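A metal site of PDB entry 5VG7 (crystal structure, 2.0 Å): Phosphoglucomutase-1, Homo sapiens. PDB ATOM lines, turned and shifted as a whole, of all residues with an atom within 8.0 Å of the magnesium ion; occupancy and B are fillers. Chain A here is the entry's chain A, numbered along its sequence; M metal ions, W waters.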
ATOM      1  N   SER A  22      32.076   3.952  11.855  1.00  0.00           N
ATOM      2  CA  SER A  22      30.679   3.625  11.573  1.00  0.00           C
ATOM      3  C   SER A  22      30.213   4.159  10.231  1.00  0.00           C
ATOM      4  O   SER A  22      29.017   4.100   9.931  1.00  0.00           O
ATOM      5  CB  SER A  22      29.777   4.158  12.694  1.00  0.00           C
ATOM      6  OG  SER A  22      30.170   5.458  13.096  1.00  0.00           O
ATOM      7  N   ARG A  25      29.073  10.026   7.589  1.00  0.00           N
ATOM      8  CA  ARG A  25      27.774  10.577   7.944  1.00  0.00           C
ATOM      9  C   ARG A  25      27.783  12.076   7.690  1.00  0.00           C
ATOM     10  O   ARG A  25      28.620  12.795   8.227  1.00  0.00           O
ATOM     11  CB  ARG A  25      27.437  10.285   9.409  1.00  0.00           C
ATOM     12  CG  ARG A  25      27.362   8.796   9.741  1.00  0.00           C
ATOM     13  CD  ARG A  25      26.930   8.559  11.172  1.00  0.00           C
ATOM     14  NE  ARG A  25      26.629   7.152  11.437  1.00  0.00           N
ATOM     15  CZ  ARG A  25      26.590   6.625  12.654  1.00  0.00           C
ATOM     16  NH1 ARG A  25      26.832   7.374  13.718  1.00  0.00           N
ATOM     17  NH2 ARG A  25      26.315   5.335  12.798  1.00  0.00           N
ATOM     18  N   ASP A  64      18.750   1.223   6.133  1.00  0.00           N
ATOM     19  CA  ASP A  64      17.782   1.295   7.218  1.00  0.00           C
ATOM     20  C   ASP A  64      16.477   1.972   6.819  1.00  0.00           C
ATOM     21  O   ASP A  64      15.614   2.179   7.681  1.00  0.00           O
ATOM     22  CB  ASP A  64      18.404   2.006   8.446  1.00  0.00           C
ATOM     23  CG  ASP A  64      18.703   3.490   8.195  1.00  0.00           C
ATOM     24  OD1 ASP A  64      18.155   4.097   7.252  1.00  0.00           O
ATOM     25  OD2 ASP A  64      19.506   4.059   9.000  1.00  0.00           O
ATOM     26  N   ARG A  66      15.966   5.084   5.596  1.00  0.00           N
ATOM     27  CA  ARG A  66      15.832   6.528   5.733  1.00  0.00           C
ATOM     28  C   ARG A  66      15.784   7.199   4.361  1.00  0.00           C
ATOM     29  O   ARG A  66      16.206   6.640   3.341  1.00  0.00           O
ATOM     30  CB  ARG A  66      16.978   7.104   6.576  1.00  0.00           C
ATOM     31  CG  ARG A  66      18.352   7.036   5.897  1.00  0.00           C
ATOM     32  CD  ARG A  66      19.471   7.489   6.824  1.00  0.00           C
ATOM     33  NE  ARG A  66      19.503   6.736   8.088  1.00  0.00           N
ATOM     34  CZ  ARG A  66      19.555   7.293   9.297  1.00  0.00           C
ATOM     35  NH1 ARG A  66      19.585   8.620   9.426  1.00  0.00           N
ATOM     36  NH2 ARG A  66      19.590   6.530  10.398  1.00  0.00           N
ATOM     37  N   THR A  98      21.593  -3.802   9.632  1.00  0.00           N
ATOM     38  CA  THR A  98      23.036  -3.993   9.711  1.00  0.00           C
ATOM     39  C   THR A  98      23.409  -5.431  10.100  1.00  0.00           C
ATOM     40  O   THR A  98      24.299  -6.005   9.453  1.00  0.00           O
ATOM     41  CB  THR A  98      23.599  -2.923  10.657  1.00  0.00           C
ATOM     42  OG1 THR A  98      23.566  -1.668   9.966  1.00  0.00           O
ATOM     43  CG2 THR A  98      25.058  -3.221  11.060  1.00  0.00           C
ATOM     44  N   PRO A  99      22.751  -6.071  11.068  1.00  0.00           N
ATOM     45  CA  PRO A  99      23.040  -7.501  11.310  1.00  0.00           C
ATOM     46  C   PRO A  99      22.725  -8.390  10.125  1.00  0.00           C
ATOM     47  O   PRO A  99      23.422  -9.388   9.896  1.00  0.00           O
ATOM     48  CB  PRO A  99      22.163  -7.847  12.531  1.00  0.00           C
ATOM     49  CG  PRO A  99      21.990  -6.511  13.253  1.00  0.00           C
ATOM     50  CD  PRO A  99      21.897  -5.494  12.138  1.00  0.00           C
ATOM     51  N   THR A 117      23.104   3.639   6.228  1.00  0.00           N
ATOM     52  CA  THR A 117      22.484   3.891   7.514  1.00  0.00           C
ATOM     53  C   THR A 117      23.300   4.951   8.228  1.00  0.00           C
ATOM     54  O   THR A 117      24.506   5.059   8.017  1.00  0.00           O
ATOM     55  CB  THR A 117      22.394   2.622   8.363  1.00  0.00           C
ATOM     56  OG1 THR A 117      21.788   2.952   9.613  1.00  0.00           O
ATOM     57  CG2 THR A 117      23.800   2.049   8.652  1.00  0.00           C
ATOM     58  N   ALA A 118      22.612   5.743   9.044  1.00  0.00           N
ATOM     59  CA  ALA A 118      23.309   6.589  10.018  1.00  0.00           C
ATOM     60  C   ALA A 118      22.832   6.182  11.415  1.00  0.00           C
ATOM     61  O   ALA A 118      22.775   6.999  12.342  1.00  0.00           O
ATOM     62  CB  ALA A 118      23.042   8.047   9.767  1.00  0.00           C
ATOM     63  N   SEP A 119      22.445   4.905  11.525  1.00  0.00           N
ATOM     64  CA  SEP A 119      22.128   4.278  12.800  1.00  0.00           C
ATOM     65  CB  SEP A 119      23.383   4.148  13.661  1.00  0.00           C
ATOM     66  OG  SEP A 119      23.170   3.232  14.718  1.00  0.00           O
ATOM     67  C   SEP A 119      21.033   5.021  13.574  1.00  0.00           C
ATOM     68  O   SEP A 119      19.917   5.116  13.105  1.00  0.00           O
ATOM     69  N   HIS A 120      21.384   5.579  14.745  1.00  0.00           N
ATOM     70  CA  HIS A 120      20.424   6.258  15.611  1.00  0.00           C
ATOM     71  C   HIS A 120      20.167   7.720  15.236  1.00  0.00           C
ATOM     72  O   HIS A 120      19.300   8.373  15.806  1.00  0.00           O
ATOM     73  CB  HIS A 120      20.907   6.203  17.054  1.00  0.00           C
ATOM     74  CG  HIS A 120      22.165   6.980  17.290  1.00  0.00           C
ATOM     75  ND1 HIS A 120      23.414   6.398  17.268  1.00  0.00           N
ATOM     76  CD2 HIS A 120      22.367   8.302  17.503  1.00  0.00           C
ATOM     77  CE1 HIS A 120      24.331   7.332  17.475  1.00  0.00           C
ATOM     78  NE2 HIS A 120      23.724   8.497  17.625  1.00  0.00           N
ATOM     79  N   ASN A 121      20.957   8.234  14.299  1.00  0.00           N
ATOM     80  CA  ASN A 121      20.794   9.634  13.921  1.00  0.00           C
ATOM     81  C   ASN A 121      19.504   9.826  13.101  1.00  0.00           C
ATOM     82  O   ASN A 121      19.094   8.924  12.362  1.00  0.00           O
ATOM     83  CB  ASN A 121      22.011  10.090  13.141  1.00  0.00           C
ATOM     84  CG  ASN A 121      23.264  10.080  13.992  1.00  0.00           C
ATOM     85  OD1 ASN A 121      23.480  10.992  14.775  1.00  0.00           O
ATOM     86  ND2 ASN A 121      24.074   9.025  13.878  1.00  0.00           N
ATOM     87  N   LYS A 132      28.263   3.204   5.053  1.00  0.00           N
ATOM     88  CA  LYS A 132      29.137   2.381   5.849  1.00  0.00           C
ATOM     89  C   LYS A 132      29.714   1.255   4.986  1.00  0.00           C
ATOM     90  O   LYS A 132      28.981   0.666   4.188  1.00  0.00           O
ATOM     91  CB  LYS A 132      28.332   1.846   7.024  1.00  0.00           C
ATOM     92  CG  LYS A 132      28.967   0.825   7.899  1.00  0.00           C
ATOM     93  CD  LYS A 132      28.088   0.704   9.150  1.00  0.00           C
ATOM     94  CE  LYS A 132      28.129  -0.682   9.735  1.00  0.00           C
ATOM     95  NZ  LYS A 132      29.514  -1.134   9.991  1.00  0.00           N
ATOM     96  N   PRO A 264      15.583   7.330  15.948  1.00  0.00           N
ATOM     97  CA  PRO A 264      15.438   5.889  16.274  1.00  0.00           C
ATOM     98  C   PRO A 264      16.631   5.461  17.130  1.00  0.00           C
ATOM     99  O   PRO A 264      17.579   4.813  16.683  1.00  0.00           O
ATOM    100  CB  PRO A 264      15.436   5.231  14.891  1.00  0.00           C
ATOM    101  CG  PRO A 264      16.447   6.114  14.105  1.00  0.00           C
ATOM    102  CD  PRO A 264      16.273   7.533  14.653  1.00  0.00           C
ATOM    103  N   ASP A 265      16.539   5.851  18.397  1.00  0.00           N
ATOM    104  CA  ASP A 265      17.617   5.693  19.369  1.00  0.00           C
ATOM    105  C   ASP A 265      16.986   5.117  20.640  1.00  0.00           C
ATOM    106  O   ASP A 265      16.175   5.805  21.293  1.00  0.00           O
ATOM    107  CB  ASP A 265      18.272   7.059  19.618  1.00  0.00           C
ATOM    108  CG  ASP A 265      19.574   6.967  20.390  1.00  0.00           C
ATOM    109  OD1 ASP A 265      19.980   5.862  20.790  1.00  0.00           O
ATOM    110  OD2 ASP A 265      20.197   8.030  20.572  1.00  0.00           O
ATOM    111  N   PRO A 266      17.261   3.847  20.997  1.00  0.00           N
ATOM    112  CA  PRO A 266      16.511   3.209  22.097  1.00  0.00           C
ATOM    113  C   PRO A 266      17.065   3.597  23.424  1.00  0.00           C
ATOM    114  O   PRO A 266      18.202   3.193  23.811  1.00  0.00           O
ATOM    115  CB  PRO A 266      16.683   1.713  21.793  1.00  0.00           C
ATOM    116  CG  PRO A 266      18.010   1.624  21.096  1.00  0.00           C
ATOM    117  CD  PRO A 266      18.168   2.900  20.312  1.00  0.00           C
ATOM    118  N   PHE A 289      14.646  -0.944  19.442  1.00  0.00           N
ATOM    119  CA  PHE A 289      15.831  -1.032  18.598  1.00  0.00           C
ATOM    120  C   PHE A 289      16.196   0.335  18.029  1.00  0.00           C
ATOM    121  O   PHE A 289      15.347   1.205  17.899  1.00  0.00           O
ATOM    122  CB  PHE A 289      15.617  -1.997  17.425  1.00  0.00           C
ATOM    123  CG  PHE A 289      15.123  -3.341  17.867  1.00  0.00           C
ATOM    124  CD1 PHE A 289      15.885  -4.105  18.749  1.00  0.00           C
ATOM    125  CD2 PHE A 289      13.905  -3.843  17.406  1.00  0.00           C
ATOM    126  CE1 PHE A 289      15.434  -5.356  19.162  1.00  0.00           C
ATOM    127  CE2 PHE A 289      13.453  -5.101  17.807  1.00  0.00           C
ATOM    128  CZ  PHE A 289      14.204  -5.851  18.706  1.00  0.00           C
ATOM    129  N   ASP A 290      17.464   0.478  17.611  1.00  0.00           N
ATOM    130  CA  ASP A 290      17.865   1.693  16.905  1.00  0.00           C
ATOM    131  C   ASP A 290      17.603   1.521  15.415  1.00  0.00           C
ATOM    132  O   ASP A 290      17.090   0.496  14.949  1.00  0.00           O
ATOM    133  CB  ASP A 290      19.324   2.070  17.181  1.00  0.00           C
ATOM    134  CG  ASP A 290      20.328   1.102  16.567  1.00  0.00           C
ATOM    135  OD1 ASP A 290      19.988  -0.071  16.239  1.00  0.00           O
ATOM    136  OD2 ASP A 290      21.501   1.534  16.407  1.00  0.00           O
ATOM    137  N   GLY A 291      17.940   2.566  14.652  1.00  0.00           N
ATOM    138  CA  GLY A 291      17.494   2.641  13.268  1.00  0.00           C
ATOM    139  C   GLY A 291      18.000   1.514  12.385  1.00  0.00           C
ATOM    140  O   GLY A 291      17.286   1.077  11.463  1.00  0.00           O
ATOM    141  N   ASP A 292      19.234   1.025  12.628  1.00  0.00           N
ATOM    142  CA  ASP A 292      19.760  -0.061  11.794  1.00  0.00           C
ATOM    143  C   ASP A 292      19.780  -1.416  12.508  1.00  0.00           C
ATOM    144  O   ASP A 292      20.242  -2.403  11.921  1.00  0.00           O
ATOM    145  CB  ASP A 292      21.167   0.251  11.245  1.00  0.00           C
ATOM    146  CG  ASP A 292      22.221   0.429  12.333  1.00  0.00           C
ATOM    147  OD1 ASP A 292      23.401   0.137  12.020  1.00  0.00           O
ATOM    148  OD2 ASP A 292      21.895   0.861  13.467  1.00  0.00           O
ATOM    149  N   GLY A 293      19.274  -1.507  13.734  1.00  0.00           N
ATOM    150  CA  GLY A 293      19.074  -2.788  14.385  1.00  0.00           C
ATOM    151  C   GLY A 293      20.242  -3.391  15.137  1.00  0.00           C
ATOM    152  O   GLY A 293      20.136  -4.550  15.557  1.00  0.00           O
ATOM    153  N   ASP A 294      21.322  -2.646  15.391  1.00  0.00           N
ATOM    154  CA  ASP A 294      22.398  -3.245  16.168  1.00  0.00           C
ATOM    155  C   ASP A 294      22.410  -2.830  17.642  1.00  0.00           C
ATOM    156  O   ASP A 294      23.247  -3.334  18.403  1.00  0.00           O
ATOM    157  CB  ASP A 294      23.764  -2.980  15.485  1.00  0.00           C
ATOM    158  CG  ASP A 294      24.204  -1.529  15.544  1.00  0.00           C
ATOM    159  OD1 ASP A 294      23.348  -0.638  15.694  1.00  0.00           O
ATOM    160  OD2 ASP A 294      25.434  -1.294  15.400  1.00  0.00           O
ATOM    161  N   ARG A 295      21.458  -1.998  18.094  1.00  0.00           N
ATOM    162  CA  ARG A 295      21.313  -1.676  19.514  1.00  0.00           C
ATOM    163  C   ARG A 295      19.921  -2.058  20.011  1.00  0.00           C
ATOM    164  O   ARG A 295      18.977  -2.213  19.228  1.00  0.00           O
ATOM    165  CB  ARG A 295      21.595  -0.163  19.771  1.00  0.00           C
ATOM    166  CG  ARG A 295      22.856   0.327  19.067  1.00  0.00           C
ATOM    167  CD  ARG A 295      23.632   1.435  19.806  1.00  0.00           C
ATOM    168  NE  ARG A 295      22.866   2.668  19.942  1.00  0.00           N
ATOM    169  CZ  ARG A 295      23.398   3.837  20.295  1.00  0.00           C
ATOM    170  NH1 ARG A 295      24.710   3.944  20.516  1.00  0.00           N
ATOM    171  NH2 ARG A 295      22.629   4.915  20.411  1.00  0.00           N
ATOM    172  N   ASN A 296      19.823  -2.291  21.320  1.00  0.00           N
ATOM    173  CA  ASN A 296      18.560  -2.701  21.932  1.00  0.00           C
ATOM    174  C   ASN A 296      18.457  -2.188  23.349  1.00  0.00           C
ATOM    175  O   ASN A 296      19.448  -2.172  24.086  1.00  0.00           O
ATOM    176  CB  ASN A 296      18.405  -4.227  21.965  1.00  0.00           C
ATOM    177  CG  ASN A 296      19.384  -4.875  22.927  1.00  0.00           C
ATOM    178  OD1 ASN A 296      19.012  -5.286  24.047  1.00  0.00           O
ATOM    179  ND2 ASN A 296      20.657  -4.951  22.516  1.00  0.00           N
ATOM    180  N   PHE A 381      23.764   0.334  25.069  1.00  0.00           N
ATOM    181  CA  PHE A 381      22.643  -0.425  24.494  1.00  0.00           C
ATOM    182  C   PHE A 381      23.134  -1.370  23.407  1.00  0.00           C
ATOM    183  O   PHE A 381      22.429  -1.629  22.428  1.00  0.00           O
ATOM    184  CB  PHE A 381      21.534   0.506  23.980  1.00  0.00           C
ATOM    185  CG  PHE A 381      20.913   1.350  25.064  1.00  0.00           C
ATOM    186  CD1 PHE A 381      19.857   0.856  25.825  1.00  0.00           C
ATOM    187  CD2 PHE A 381      21.440   2.605  25.370  1.00  0.00           C
ATOM    188  CE1 PHE A 381      19.316   1.610  26.873  1.00  0.00           C
ATOM    189  CE2 PHE A 381      20.892   3.388  26.403  1.00  0.00           C
ATOM    190  CZ  PHE A 381      19.842   2.894  27.156  1.00  0.00           C
ATOM    191  N   GLU A 390      28.623  -7.846  13.598  1.00  0.00           N
ATOM    192  CA  GLU A 390      28.068  -6.589  14.091  1.00  0.00           C
ATOM    193  C   GLU A 390      27.269  -6.942  15.336  1.00  0.00           C
ATOM    194  O   GLU A 390      26.854  -8.095  15.516  1.00  0.00           O
ATOM    195  CB  GLU A 390      27.159  -5.875  13.057  1.00  0.00           C
ATOM    196  CG  GLU A 390      27.831  -5.424  11.748  1.00  0.00           C
ATOM    197  CD  GLU A 390      28.497  -4.048  11.886  1.00  0.00           C
ATOM    198  OE1 GLU A 390      28.485  -3.482  12.997  1.00  0.00           O
ATOM    199  OE2 GLU A 390      29.035  -3.530  10.885  1.00  0.00           O
ATOM    200  N   LYS A 391      27.037  -5.951  16.208  1.00  0.00           N
ATOM    201  CA  LYS A 391      26.068  -6.168  17.282  1.00  0.00           C
ATOM    202  C   LYS A 391      24.662  -6.359  16.692  1.00  0.00           C
ATOM    203  O   LYS A 391      24.408  -6.066  15.520  1.00  0.00           O
ATOM    204  CB  LYS A 391      26.112  -5.011  18.285  1.00  0.00           C
ATOM    205  CG  LYS A 391      27.479  -4.894  18.965  1.00  0.00           C
ATOM    206  CD  LYS A 391      27.600  -3.648  19.843  1.00  0.00           C
ATOM    207  CE  LYS A 391      27.161  -2.372  19.135  1.00  0.00           C
ATOM    208  NZ  LYS A 391      28.113  -1.831  18.111  1.00  0.00           N
HETATM  209 MG    MG M   1      23.100   1.239  15.140  1.00  0.00          MG
HETATM  210  O   HOH W   1      24.434   1.849  16.738  1.00  0.00           O
HETATM  211  O   HOH W   2      24.970   1.107  13.813  1.00  0.00           O
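OD1 of Asp 294 is bound to the magnesium ion, 2.0 Å away.
The magnesium ion is bound by OG of SEP 119 (2.0 Å).
The magnesium ion is bound by the side-chain carboxylate (OD2) of Asp 290 (2.1 Å).
The side-chain carboxylate (OD2) of Asp 292 is bound to the magnesium ion, 2.1 Å away.
Water W1 is bound to the magnesium ion, at 2.2 Å.
Water W2 binds the magnesium ion.
The magnesium ion has six donor atoms within binding distance.
Within 4 Å of the magnesium ion: SEP 119, Asp 290, Asp 292 and Asp 294.
The nearest printed residue that does not touch the magnesium ion is Arg 295 (4.04 Å).
Water W2 bridges the side-chain carboxylate (OD1) of Asp 292 and the side-chain carboxylate (OD2) of Asp 294.
NZ of Lys 391 is in salt-bridge range of OD2 of Asp 294, 3.8 Å away.
The side-chain hydroxyl (OG1) of Thr 117 is in hydrogen-bond range of N of SEP 119 (2.8 Å).
The guanidinium group (NH2) of Arg 66 is in hydrogen-bond range of O of SEP 119 (3.1 Å).
The side-chain carboxylate (OD1) of Asp 290 sits at hydrogen-bond distance from the backbone NH (N) of Arg 295 (3.1 Å).
The side-chain carboxylate (OD1) of Asp 290 is in hydrogen-bond range of the backbone NH (N) of Gly 293.
The side-chain carboxylate of Asp 292 is in hydrogen-bond range of the side-chain hydroxyl of Thr 98, at 2.7 Å.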
